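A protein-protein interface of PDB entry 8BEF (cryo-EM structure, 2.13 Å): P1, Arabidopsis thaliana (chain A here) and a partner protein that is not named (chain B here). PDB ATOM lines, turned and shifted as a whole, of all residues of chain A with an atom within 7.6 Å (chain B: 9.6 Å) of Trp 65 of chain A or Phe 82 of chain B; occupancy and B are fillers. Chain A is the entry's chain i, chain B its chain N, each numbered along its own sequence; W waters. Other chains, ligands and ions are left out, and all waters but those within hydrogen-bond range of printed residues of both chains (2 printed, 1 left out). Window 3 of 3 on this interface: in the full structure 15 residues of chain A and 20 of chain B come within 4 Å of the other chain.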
ATOM      1  N   ASN A  60      13.942  18.053  20.975  1.00  0.00           N
ATOM      2  CA  ASN A  60      12.497  18.174  21.125  1.00  0.00           C
ATOM      3  C   ASN A  60      11.811  16.821  20.965  1.00  0.00           C
ATOM      4  O   ASN A  60      10.711  16.724  20.418  1.00  0.00           O
ATOM      5  CB  ASN A  60      11.930  19.183  20.129  1.00  0.00           C
ATOM      6  CG  ASN A  60      12.330  20.611  20.453  1.00  0.00           C
ATOM      7  OD1 ASN A  60      12.643  20.939  21.597  1.00  0.00           O
ATOM      8  ND2 ASN A  60      12.319  21.470  19.438  1.00  0.00           N
ATOM      9  N   ALA A  61      12.463  15.760  21.441  1.00  0.00           N
ATOM     10  CA  ALA A  61      11.923  14.416  21.259  1.00  0.00           C
ATOM     11  C   ALA A  61      10.572  14.254  21.949  1.00  0.00           C
ATOM     12  O   ALA A  61       9.648  13.666  21.377  1.00  0.00           O
ATOM     13  CB  ALA A  61      12.919  13.376  21.774  1.00  0.00           C
ATOM     14  N   GLN A  62      10.432  14.775  23.171  1.00  0.00           N
ATOM     15  CA  GLN A  62       9.189  14.575  23.911  1.00  0.00           C
ATOM     16  C   GLN A  62       8.023  15.306  23.249  1.00  0.00           C
ATOM     17  O   GLN A  62       6.894  14.804  23.245  1.00  0.00           O
ATOM     18  CB  GLN A  62       9.359  15.012  25.370  1.00  0.00           C
ATOM     19  CG  GLN A  62       8.050  15.133  26.148  1.00  0.00           C
ATOM     20  CD  GLN A  62       8.249  15.410  27.633  1.00  0.00           C
ATOM     21  OE1 GLN A  62       9.159  16.136  28.028  1.00  0.00           O
ATOM     22  NE2 GLN A  62       7.386  14.834  28.460  1.00  0.00           N
ATOM     23  N   LEU A  63       8.279  16.484  22.674  1.00  0.00           N
ATOM     24  CA  LEU A  63       7.227  17.226  21.985  1.00  0.00           C
ATOM     25  C   LEU A  63       6.627  16.450  20.821  1.00  0.00           C
ATOM     26  O   LEU A  63       5.485  16.718  20.438  1.00  0.00           O
ATOM     27  CB  LEU A  63       7.766  18.565  21.483  1.00  0.00           C
ATOM     28  CG  LEU A  63       7.963  19.686  22.508  1.00  0.00           C
ATOM     29  CD1 LEU A  63       7.967  21.027  21.813  1.00  0.00           C
ATOM     30  CD2 LEU A  63       6.895  19.649  23.581  1.00  0.00           C
ATOM     31  N   ARG A  64       7.363  15.500  20.244  1.00  0.00           N
ATOM     32  CA  ARG A  64       6.854  14.712  19.130  1.00  0.00           C
ATOM     33  C   ARG A  64       6.411  13.312  19.530  1.00  0.00           C
ATOM     34  O   ARG A  64       5.572  12.728  18.838  1.00  0.00           O
ATOM     35  CB  ARG A  64       7.912  14.603  18.029  1.00  0.00           C
ATOM     36  CG  ARG A  64       8.674  15.888  17.789  1.00  0.00           C
ATOM     37  CD  ARG A  64       9.091  16.013  16.336  1.00  0.00           C
ATOM     38  NE  ARG A  64      10.074  15.005  15.954  1.00  0.00           N
ATOM     39  CZ  ARG A  64      11.331  14.981  16.376  1.00  0.00           C
ATOM     40  NH1 ARG A  64      11.800  15.894  17.210  1.00  0.00           N
ATOM     41  NH2 ARG A  64      12.139  14.015  15.949  1.00  0.00           N
ATOM     42  N   TRP A  65       6.950  12.766  20.619  1.00  0.00           N
ATOM     43  CA  TRP A  65       6.565  11.429  21.058  1.00  0.00           C
ATOM     44  C   TRP A  65       5.285  11.465  21.883  1.00  0.00           C
ATOM     45  O   TRP A  65       4.344  10.717  21.611  1.00  0.00           O
ATOM     46  CB  TRP A  65       7.700  10.795  21.862  1.00  0.00           C
ATOM     47  CG  TRP A  65       7.341   9.482  22.481  1.00  0.00           C
ATOM     48  CD1 TRP A  65       7.237   9.205  23.812  1.00  0.00           C
ATOM     49  CD2 TRP A  65       7.057   8.259  21.794  1.00  0.00           C
ATOM     50  NE1 TRP A  65       6.894   7.889  23.998  1.00  0.00           N
ATOM     51  CE2 TRP A  65       6.779   7.285  22.775  1.00  0.00           C
ATOM     52  CE3 TRP A  65       7.000   7.894  20.447  1.00  0.00           C
ATOM     53  CZ2 TRP A  65       6.451   5.972  22.449  1.00  0.00           C
ATOM     54  CZ3 TRP A  65       6.677   6.587  20.126  1.00  0.00           C
ATOM     55  CH2 TRP A  65       6.407   5.644  21.122  1.00  0.00           C
ATOM     56  N   ASP A  66       5.236  12.341  22.884  1.00  0.00           N
ATOM     57  CA  ASP A  66       4.104  12.380  23.806  1.00  0.00           C
ATOM     58  C   ASP A  66       2.744  12.533  23.129  1.00  0.00           C
ATOM     59  O   ASP A  66       1.784  11.903  23.605  1.00  0.00           O
ATOM     60  CB  ASP A  66       4.329  13.492  24.843  1.00  0.00           C
ATOM     61  CG  ASP A  66       5.142  13.017  26.040  1.00  0.00           C
ATOM     62  OD1 ASP A  66       5.696  11.901  25.978  1.00  0.00           O
ATOM     63  OD2 ASP A  66       5.226  13.755  27.041  1.00  0.00           O
ATOM     64  N   PRO A  67       2.570  13.334  22.068  1.00  0.00           N
ATOM     65  CA  PRO A  67       1.261  13.336  21.391  1.00  0.00           C
ATOM     66  C   PRO A  67       0.849  11.970  20.869  1.00  0.00           C
ATOM     67  O   PRO A  67      -0.351  11.692  20.783  1.00  0.00           O
ATOM     68  CB  PRO A  67       1.442  14.344  20.245  1.00  0.00           C
ATOM     69  CG  PRO A  67       2.592  15.190  20.631  1.00  0.00           C
ATOM     70  CD  PRO A  67       3.446  14.420  21.592  1.00  0.00           C
ATOM     71  N   GLN A  68       1.809  11.107  20.522  1.00  0.00           N
ATOM     72  CA  GLN A  68       1.471   9.785  20.008  1.00  0.00           C
ATOM     73  C   GLN A  68       0.929   8.855  21.091  1.00  0.00           C
ATOM     74  O   GLN A  68       0.245   7.881  20.762  1.00  0.00           O
ATOM     75  CB  GLN A  68       2.696   9.148  19.338  1.00  0.00           C
ATOM     76  CG  GLN A  68       3.130   9.819  18.039  1.00  0.00           C
ATOM     77  CD  GLN A  68       4.432   9.250  17.493  1.00  0.00           C
ATOM     78  OE1 GLN A  68       4.522   8.063  17.187  1.00  0.00           O
ATOM     79  NE2 GLN A  68       5.449  10.096  17.379  1.00  0.00           N
ATOM     80  N   ILE A  69       1.222   9.121  22.363  1.00  0.00           N
ATOM     81  CA  ILE A  69       0.716   8.325  23.476  1.00  0.00           C
ATOM     82  C   ILE A  69      -0.316   9.088  24.297  1.00  0.00           C
ATOM     83  O   ILE A  69      -0.629   8.683  25.419  1.00  0.00           O
ATOM     84  CB  ILE A  69       1.855   7.824  24.381  1.00  0.00           C
ATOM     85  CG1 ILE A  69       2.758   8.989  24.803  1.00  0.00           C
ATOM     86  CG2 ILE A  69       2.630   6.697  23.704  1.00  0.00           C
ATOM     87  CD1 ILE A  69       3.642   8.688  25.995  1.00  0.00           C
ATOM     88  N   SER A  70      -0.856  10.184  23.762  1.00  0.00           N
ATOM     89  CA  SER A  70      -1.737  11.046  24.542  1.00  0.00           C
ATOM     90  C   SER A  70      -3.069  10.386  24.877  1.00  0.00           C
ATOM     91  O   SER A  70      -3.762  10.851  25.786  1.00  0.00           O
ATOM     92  CB  SER A  70      -1.975  12.362  23.794  1.00  0.00           C
ATOM     93  OG  SER A  70      -2.760  12.154  22.637  1.00  0.00           O
ATOM     94  N   ARG A  75      -2.413   8.307  31.363  1.00  0.00           N
ATOM     95  CA  ARG A  75      -1.996   9.695  31.204  1.00  0.00           C
ATOM     96  C   ARG A  75      -3.066  10.552  30.528  1.00  0.00           C
ATOM     97  O   ARG A  75      -2.757  11.649  30.053  1.00  0.00           O
ATOM     98  CB  ARG A  75      -0.680   9.782  30.416  1.00  0.00           C
ATOM     99  CG  ARG A  75      -0.754   9.235  29.003  1.00  0.00           C
ATOM    100  CD  ARG A  75       0.634   9.046  28.412  1.00  0.00           C
ATOM    101  NE  ARG A  75       1.289  10.313  28.113  1.00  0.00           N
ATOM    102  CZ  ARG A  75       2.298  10.818  28.807  1.00  0.00           C
ATOM    103  NH1 ARG A  75       2.795  10.190  29.861  1.00  0.00           N
ATOM    104  NH2 ARG A  75       2.820  11.982  28.438  1.00  0.00           N
ATOM    105  N   MET B  12       7.667  -3.907  14.160  1.00  0.00           N
ATOM    106  CA  MET B  12       8.079  -4.026  15.557  1.00  0.00           C
ATOM    107  C   MET B  12       9.522  -4.508  15.695  1.00  0.00           C
ATOM    108  O   MET B  12      10.306  -3.930  16.447  1.00  0.00           O
ATOM    109  CB  MET B  12       7.142  -4.971  16.311  1.00  0.00           C
ATOM    110  CG  MET B  12       7.661  -5.391  17.678  1.00  0.00           C
ATOM    111  SD  MET B  12       7.817  -4.015  18.831  1.00  0.00           S
ATOM    112  CE  MET B  12       6.139  -3.895  19.433  1.00  0.00           C
ATOM    113  N   PHE B  13       9.864  -5.573  14.965  1.00  0.00           N
ATOM    114  CA  PHE B  13      11.216  -6.120  15.040  1.00  0.00           C
ATOM    115  C   PHE B  13      12.262  -5.084  14.646  1.00  0.00           C
ATOM    116  O   PHE B  13      13.335  -5.017  15.255  1.00  0.00           O
ATOM    117  CB  PHE B  13      11.336  -7.359  14.149  1.00  0.00           C
ATOM    118  CG  PHE B  13      12.675  -8.040  14.234  1.00  0.00           C
ATOM    119  CD1 PHE B  13      13.717  -7.669  13.395  1.00  0.00           C
ATOM    120  CD2 PHE B  13      12.894  -9.047  15.160  1.00  0.00           C
ATOM    121  CE1 PHE B  13      14.950  -8.291  13.481  1.00  0.00           C
ATOM    122  CE2 PHE B  13      14.122  -9.674  15.250  1.00  0.00           C
ATOM    123  CZ  PHE B  13      15.154  -9.295  14.408  1.00  0.00           C
ATOM    124  N   ASN B  14      11.971  -4.274  13.626  1.00  0.00           N
ATOM    125  CA  ASN B  14      12.965  -3.326  13.128  1.00  0.00           C
ATOM    126  C   ASN B  14      13.293  -2.249  14.152  1.00  0.00           C
ATOM    127  O   ASN B  14      14.379  -1.660  14.098  1.00  0.00           O
ATOM    128  CB  ASN B  14      12.483  -2.691  11.825  1.00  0.00           C
ATOM    129  CG  ASN B  14      12.589  -3.636  10.648  1.00  0.00           C
ATOM    130  OD1 ASN B  14      13.364  -4.588  10.675  1.00  0.00           O
ATOM    131  ND2 ASN B  14      11.806  -3.379   9.608  1.00  0.00           N
ATOM    132  N   LEU B  15      12.375  -1.970  15.083  1.00  0.00           N
ATOM    133  CA  LEU B  15      12.683  -1.032  16.159  1.00  0.00           C
ATOM    134  C   LEU B  15      13.920  -1.459  16.934  1.00  0.00           C
ATOM    135  O   LEU B  15      14.699  -0.609  17.376  1.00  0.00           O
ATOM    136  CB  LEU B  15      11.497  -0.903  17.116  1.00  0.00           C
ATOM    137  CG  LEU B  15      10.102  -0.650  16.548  1.00  0.00           C
ATOM    138  CD1 LEU B  15       9.061  -0.893  17.625  1.00  0.00           C
ATOM    139  CD2 LEU B  15       9.991   0.758  15.998  1.00  0.00           C
ATOM    140  N   PHE B  16      14.128  -2.765  17.087  1.00  0.00           N
ATOM    141  CA  PHE B  16      15.229  -3.280  17.888  1.00  0.00           C
ATOM    142  C   PHE B  16      16.565  -3.245  17.157  1.00  0.00           C
ATOM    143  O   PHE B  16      17.569  -3.689  17.722  1.00  0.00           O
ATOM    144  CB  PHE B  16      14.905  -4.702  18.362  1.00  0.00           C
ATOM    145  CG  PHE B  16      13.769  -4.757  19.348  1.00  0.00           C
ATOM    146  CD1 PHE B  16      12.454  -4.758  18.913  1.00  0.00           C
ATOM    147  CD2 PHE B  16      14.016  -4.780  20.713  1.00  0.00           C
ATOM    148  CE1 PHE B  16      11.405  -4.793  19.817  1.00  0.00           C
ATOM    149  CE2 PHE B  16      12.971  -4.815  21.625  1.00  0.00           C
ATOM    150  CZ  PHE B  16      11.666  -4.821  21.177  1.00  0.00           C
ATOM    151  N   LEU B  17      16.604  -2.722  15.928  1.00  0.00           N
ATOM    152  CA  LEU B  17      17.881  -2.478  15.271  1.00  0.00           C
ATOM    153  C   LEU B  17      18.725  -1.485  16.059  1.00  0.00           C
ATOM    154  O   LEU B  17      19.957  -1.533  15.997  1.00  0.00           O
ATOM    155  CB  LEU B  17      17.657  -1.972  13.846  1.00  0.00           C
ATOM    156  CG  LEU B  17      17.229  -3.028  12.826  1.00  0.00           C
ATOM    157  CD1 LEU B  17      16.814  -2.374  11.514  1.00  0.00           C
ATOM    158  CD2 LEU B  17      18.344  -4.036  12.607  1.00  0.00           C
ATOM    159  N   ALA B  18      18.080  -0.593  16.816  1.00  0.00           N
ATOM    160  CA  ALA B  18      18.806   0.350  17.659  1.00  0.00           C
ATOM    161  C   ALA B  18      19.581  -0.336  18.777  1.00  0.00           C
ATOM    162  O   ALA B  18      20.466   0.288  19.370  1.00  0.00           O
ATOM    163  CB  ALA B  18      17.838   1.372  18.260  1.00  0.00           C
ATOM    164  N   VAL B  19      19.268  -1.593  19.090  1.00  0.00           N
ATOM    165  CA  VAL B  19      19.943  -2.291  20.180  1.00  0.00           C
ATOM    166  C   VAL B  19      20.491  -3.640  19.727  1.00  0.00           C
ATOM    167  O   VAL B  19      20.675  -4.543  20.548  1.00  0.00           O
ATOM    168  CB  VAL B  19      19.006  -2.477  21.391  1.00  0.00           C
ATOM    169  CG1 VAL B  19      18.836  -1.169  22.143  1.00  0.00           C
ATOM    170  CG2 VAL B  19      17.663  -3.043  20.958  1.00  0.00           C
ATOM    171  N   THR B  77      20.380   4.880  15.377  1.00  0.00           N
ATOM    172  CA  THR B  77      19.483   5.998  15.636  1.00  0.00           C
ATOM    173  C   THR B  77      18.055   5.734  15.179  1.00  0.00           C
ATOM    174  O   THR B  77      17.218   6.637  15.255  1.00  0.00           O
ATOM    175  CB  THR B  77      20.003   7.261  14.951  1.00  0.00           C
ATOM    176  OG1 THR B  77      20.140   7.013  13.550  1.00  0.00           O
ATOM    177  CG2 THR B  77      21.353   7.656  15.527  1.00  0.00           C
ATOM    178  N   ILE B  78      17.761   4.531  14.686  1.00  0.00           N
ATOM    179  CA  ILE B  78      16.410   4.222  14.243  1.00  0.00           C
ATOM    180  C   ILE B  78      15.458   4.245  15.435  1.00  0.00           C
ATOM    181  O   ILE B  78      15.840   3.953  16.576  1.00  0.00           O
ATOM    182  CB  ILE B  78      16.376   2.862  13.520  1.00  0.00           C
ATOM    183  CG1 ILE B  78      15.412   2.908  12.335  1.00  0.00           C
ATOM    184  CG2 ILE B  78      15.977   1.735  14.468  1.00  0.00           C
ATOM    185  CD1 ILE B  78      15.229   1.566  11.657  1.00  0.00           C
ATOM    186  N   ALA B  79      14.207   4.629  15.166  1.00  0.00           N
ATOM    187  CA  ALA B  79      13.135   4.621  16.163  1.00  0.00           C
ATOM    188  C   ALA B  79      13.506   5.427  17.406  1.00  0.00           C
ATOM    189  O   ALA B  79      13.215   5.027  18.535  1.00  0.00           O
ATOM    190  CB  ALA B  79      12.749   3.189  16.542  1.00  0.00           C
ATOM    191  N   HIS B  80      14.149   6.579  17.198  1.00  0.00           N
ATOM    192  CA  HIS B  80      14.674   7.343  18.326  1.00  0.00           C
ATOM    193  C   HIS B  80      13.565   7.871  19.230  1.00  0.00           C
ATOM    194  O   HIS B  80      13.769   7.997  20.440  1.00  0.00           O
ATOM    195  CB  HIS B  80      15.556   8.494  17.833  1.00  0.00           C
ATOM    196  CG  HIS B  80      14.806   9.585  17.135  1.00  0.00           C
ATOM    197  ND1 HIS B  80      14.035   9.363  16.017  1.00  0.00           N
ATOM    198  CD2 HIS B  80      14.710  10.910  17.400  1.00  0.00           C
ATOM    199  CE1 HIS B  80      13.499  10.503  15.619  1.00  0.00           C
ATOM    200  NE2 HIS B  80      13.891  11.456  16.443  1.00  0.00           N
ATOM    201  N   LEU B  81      12.395   8.187  18.672  1.00  0.00           N
ATOM    202  CA  LEU B  81      11.281   8.614  19.513  1.00  0.00           C
ATOM    203  C   LEU B  81      10.793   7.478  20.404  1.00  0.00           C
ATOM    204  O   LEU B  81      10.501   7.693  21.584  1.00  0.00           O
ATOM    205  CB  LEU B  81      10.140   9.148  18.651  1.00  0.00           C
ATOM    206  CG  LEU B  81      10.454  10.389  17.815  1.00  0.00           C
ATOM    207  CD1 LEU B  81       9.198  10.892  17.117  1.00  0.00           C
ATOM    208  CD2 LEU B  81      11.077  11.478  18.672  1.00  0.00           C
ATOM    209  N   PHE B  82      10.696   6.266  19.853  1.00  0.00           N
ATOM    210  CA  PHE B  82      10.257   5.119  20.641  1.00  0.00           C
ATOM    211  C   PHE B  82      11.237   4.815  21.769  1.00  0.00           C
ATOM    212  O   PHE B  82      10.825   4.470  22.881  1.00  0.00           O
ATOM    213  CB  PHE B  82      10.075   3.905  19.725  1.00  0.00           C
ATOM    214  CG  PHE B  82       9.799   2.619  20.452  1.00  0.00           C
ATOM    215  CD1 PHE B  82       8.502   2.261  20.783  1.00  0.00           C
ATOM    216  CD2 PHE B  82      10.832   1.753  20.779  1.00  0.00           C
ATOM    217  CE1 PHE B  82       8.241   1.073  21.441  1.00  0.00           C
ATOM    218  CE2 PHE B  82      10.578   0.568  21.440  1.00  0.00           C
ATOM    219  CZ  PHE B  82       9.280   0.227  21.770  1.00  0.00           C
ATOM    220  N   TRP B  83      12.534   4.943  21.504  1.00  0.00           N
ATOM    221  CA  TRP B  83      13.568   4.657  22.488  1.00  0.00           C
ATOM    222  C   TRP B  83      13.941   5.864  23.339  1.00  0.00           C
ATOM    223  O   TRP B  83      14.824   5.745  24.193  1.00  0.00           O
ATOM    224  CB  TRP B  83      14.831   4.139  21.791  1.00  0.00           C
ATOM    225  CG  TRP B  83      14.669   2.820  21.121  1.00  0.00           C
ATOM    226  CD1 TRP B  83      14.686   2.575  19.782  1.00  0.00           C
ATOM    227  CD2 TRP B  83      14.480   1.553  21.759  1.00  0.00           C
ATOM    228  NE1 TRP B  83      14.514   1.238  19.544  1.00  0.00           N
ATOM    229  CE2 TRP B  83      14.388   0.585  20.740  1.00  0.00           C
ATOM    230  CE3 TRP B  83      14.380   1.143  23.091  1.00  0.00           C
ATOM    231  CZ2 TRP B  83      14.196  -0.767  21.011  1.00  0.00           C
ATOM    232  CZ3 TRP B  83      14.192  -0.203  23.359  1.00  0.00           C
ATOM    233  CH2 TRP B  83      14.102  -1.141  22.323  1.00  0.00           C
ATOM    234  N   ASN B  84      13.294   7.014  23.132  1.00  0.00           N
ATOM    235  CA  ASN B  84      13.803   8.263  23.693  1.00  0.00           C
ATOM    236  C   ASN B  84      13.826   8.240  25.217  1.00  0.00           C
ATOM    237  O   ASN B  84      14.772   8.743  25.835  1.00  0.00           O
ATOM    238  CB  ASN B  84      12.973   9.446  23.202  1.00  0.00           C
ATOM    239  CG  ASN B  84      13.338  10.734  23.908  1.00  0.00           C
ATOM    240  OD1 ASN B  84      14.463  11.218  23.794  1.00  0.00           O
ATOM    241  ND2 ASN B  84      12.394  11.288  24.652  1.00  0.00           N
ATOM    242  N   ASN B  85      12.797   7.678  25.842  1.00  0.00           N
ATOM    243  CA  ASN B  85      12.726   7.654  27.296  1.00  0.00           C
ATOM    244  C   ASN B  85      13.562   6.540  27.912  1.00  0.00           C
ATOM    245  O   ASN B  85      13.502   6.342  29.129  1.00  0.00           O
ATOM    246  CB  ASN B  85      11.270   7.538  27.751  1.00  0.00           C
ATOM    247  CG  ASN B  85      10.496   8.825  27.538  1.00  0.00           C
ATOM    248  OD1 ASN B  85       9.417   8.828  26.953  1.00  0.00           O
ATOM    249  ND2 ASN B  85      11.066   9.932  27.990  1.00  0.00           N
ATOM    250  N   LEU B  86      14.338   5.822  27.106  1.00  0.00           N
ATOM    251  CA  LEU B  86      15.210   4.753  27.576  1.00  0.00           C
ATOM    252  C   LEU B  86      16.688   5.042  27.381  1.00  0.00           C
ATOM    253  O   LEU B  86      17.487   4.736  28.265  1.00  0.00           O
ATOM    254  CB  LEU B  86      14.867   3.439  26.868  1.00  0.00           C
ATOM    255  CG  LEU B  86      13.552   2.786  27.291  1.00  0.00           C
ATOM    256  CD1 LEU B  86      13.263   3.068  28.761  1.00  0.00           C
ATOM    257  CD2 LEU B  86      12.398   3.231  26.404  1.00  0.00           C
ATOM    258  N   PHE B  87      17.072   5.613  26.243  1.00  0.00           N
ATOM    259  CA  PHE B  87      18.464   5.944  25.957  1.00  0.00           C
ATOM    260  C   PHE B  87      18.491   6.884  24.755  1.00  0.00           C
ATOM    261  O   PHE B  87      17.456   7.189  24.156  1.00  0.00           O
ATOM    262  CB  PHE B  87      19.301   4.684  25.715  1.00  0.00           C
ATOM    263  CG  PHE B  87      18.750   3.782  24.652  1.00  0.00           C
ATOM    264  CD1 PHE B  87      18.902   4.087  23.308  1.00  0.00           C
ATOM    265  CD2 PHE B  87      18.081   2.620  24.998  1.00  0.00           C
ATOM    266  CE1 PHE B  87      18.392   3.255  22.333  1.00  0.00           C
ATOM    267  CE2 PHE B  87      17.574   1.782  24.025  1.00  0.00           C
ATOM    268  CZ  PHE B  87      17.727   2.101  22.693  1.00  0.00           C
ATOM    269  N   ARG B  88      19.694   7.336  24.402  1.00  0.00           N
ATOM    270  CA  ARG B  88      19.898   8.225  23.261  1.00  0.00           C
ATOM    271  C   ARG B  88      21.216   7.876  22.588  1.00  0.00           C
ATOM    272  O   ARG B  88      22.280   8.024  23.197  1.00  0.00           O
ATOM    273  CB  ARG B  88      19.903   9.695  23.690  1.00  0.00           C
ATOM    274  CG  ARG B  88      19.933  10.667  22.520  1.00  0.00           C
ATOM    275  CD  ARG B  88      19.527  12.063  22.944  1.00  0.00           C
ATOM    276  NE  ARG B  88      18.079  12.213  23.011  1.00  0.00           N
ATOM    277  CZ  ARG B  88      17.453  13.377  23.103  1.00  0.00           C
ATOM    278  NH1 ARG B  88      18.120  14.521  23.115  1.00  0.00           N
ATOM    279  NH2 ARG B  88      16.127  13.395  23.195  1.00  0.00           N
ATOM    280  N   HIS B 205      14.738  12.965  32.848  1.00  0.00           N
ATOM    281  CA  HIS B 205      15.275  12.899  31.496  1.00  0.00           C
ATOM    282  C   HIS B 205      16.203  14.082  31.234  1.00  0.00           C
ATOM    283  O   HIS B 205      15.930  15.210  31.655  1.00  0.00           O
ATOM    284  CB  HIS B 205      14.126  12.876  30.485  1.00  0.00           C
ATOM    285  CG  HIS B 205      14.538  12.502  29.096  1.00  0.00           C
ATOM    286  ND1 HIS B 205      15.055  13.413  28.201  1.00  0.00           N
ATOM    287  CD2 HIS B 205      14.497  11.316  28.444  1.00  0.00           C
ATOM    288  CE1 HIS B 205      15.315  12.805  27.058  1.00  0.00           C
ATOM    289  NE2 HIS B 205      14.986  11.532  27.178  1.00  0.00           N
ATOM    290  N   GLN B 208      14.693  17.242  29.512  1.00  0.00           N
ATOM    291  CA  GLN B 208      13.866  18.035  30.414  1.00  0.00           C
ATOM    292  C   GLN B 208      14.728  18.828  31.386  1.00  0.00           C
ATOM    293  O   GLN B 208      14.468  20.008  31.637  1.00  0.00           O
ATOM    294  CB  GLN B 208      12.901  17.123  31.171  1.00  0.00           C
ATOM    295  CG  GLN B 208      12.032  16.241  30.288  1.00  0.00           C
ATOM    296  CD  GLN B 208      11.345  15.126  31.061  1.00  0.00           C
ATOM    297  OE1 GLN B 208      11.812  14.708  32.119  1.00  0.00           O
ATOM    298  NE2 GLN B 208      10.228  14.642  30.533  1.00  0.00           N
HETATM  299  O   HOH W   1       7.175   6.786  26.534  1.00  0.00           O
HETATM  300  O   HOH W   2       8.563  11.739  26.170  1.00  0.00           O
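NH1 of Arg 64 of chain A lies close to O of Asn 60 of chain A.
A ring nitrogen (NE2) of His 205 of chain B lies within hydrogen-bond range of the backbone carbonyl oxygen (O) of Asn 84 of chain B (3.1 Å).
NH2 of Arg 88 of chain B sits at hydrogen-bond distance from OD1 of Asn 84 of chain B (2.8 Å).
The backbone carbonyl oxygen (O) of Arg 64 of chain A is in hydrogen-bond range of the side-chain amide nitrogen (NE2) of Gln 68 of chain A, 3.0 Å away.
OE1 of Gln 208 of chain B lies close to N of His 205 of chain B (3.5 Å).
The side-chain amide nitrogen of Gln 62 of chain A is in hydrogen-bond range of the side-chain carboxylate of Asp 66 of chain A (2.8 Å).
Water W1 bridges NE1 of Trp 65 of chain A (2.8 Å) and OD1 of Asn 85 of chain B (3.1 Å).
Water W2 bridges the side-chain carboxylate (OD1) of Asp 66 of chain A and the side-chain amide oxygen (OD1) of Asn 85 of chain B.
Of the 12 printed residues of chain A, 5 touch a printed residue of chain B.
Hydrophobic or aromatic side chains of chain A within 4 Å of the printed part of chain B: Ala 61 and Trp 65.
Hydrophobic or aromatic side chains of chain B that line the printed part of chain A: His 80, Leu 81 and Phe 82.
Among the printed residues, 10 pairs touch across the chains.
Among the printed residues, merely in contact across the chains: Ala 61 of chain A with Asn 84 of chain B, Trp 65 of chain A with Leu 81 of chain B, Ala 61 of chain A with Arg 88 of chain B, Ala 61 of chain A with Leu 81 of chain B, Gln 68 of chain A with Leu 81 of chain B, Trp 65 of chain A with Asn 85 of chain B, Arg 64 of chain A with Leu 81 of chain B and Trp 65 of chain A with Phe 82 of chain B.
Trp 65 of chain A touches just these residues of chain B: Leu 81, Phe 82 and Asn 85.
Of the printed residues of chain A, Phe 82 of chain B touches Trp 65 (3.9 Å).
No residue of chain B comes within 4 Å of Pro 67 of chain A.
Of chain B, only Leu 81 comes within 4 Å of Gln 68 of chain A.
Of the printed residues of chain B, Arg 64 of chain A touches His 80 (3.1 Å) and Leu 81 (3.9 Å).
Of the printed residues of chain A, Asn 85 of chain B touches Trp 65.
Of the printed residues of chain A, Arg 88 of chain B touches Ala 61 (3.5 Å).
Printed residues of chain A within 4 Å of Asn 84 of chain B: Ala 61.
Ser 70 of chain A touches none of the printed residues of chain B.
Phe 16 of chain B touches none of the printed residues of chain A.
The nearest residue of chain A that does not touch Phe 82 of chain B is Gln 68 of chain A (7.0 Å).
The nearest printed residue of chain A that does not touch Arg 88 of chain B is Asn 60 of chain A (5.6 Å).
NH2 of Arg 64 of chain A sits at hydrogen-bond distance from NE2 of His 80 of chain B, 3.1 Å away.
NE2 of Gln 208 of chain B is in hydrogen-bond range of OE1 of Gln 62 of chain A (3.1 Å).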
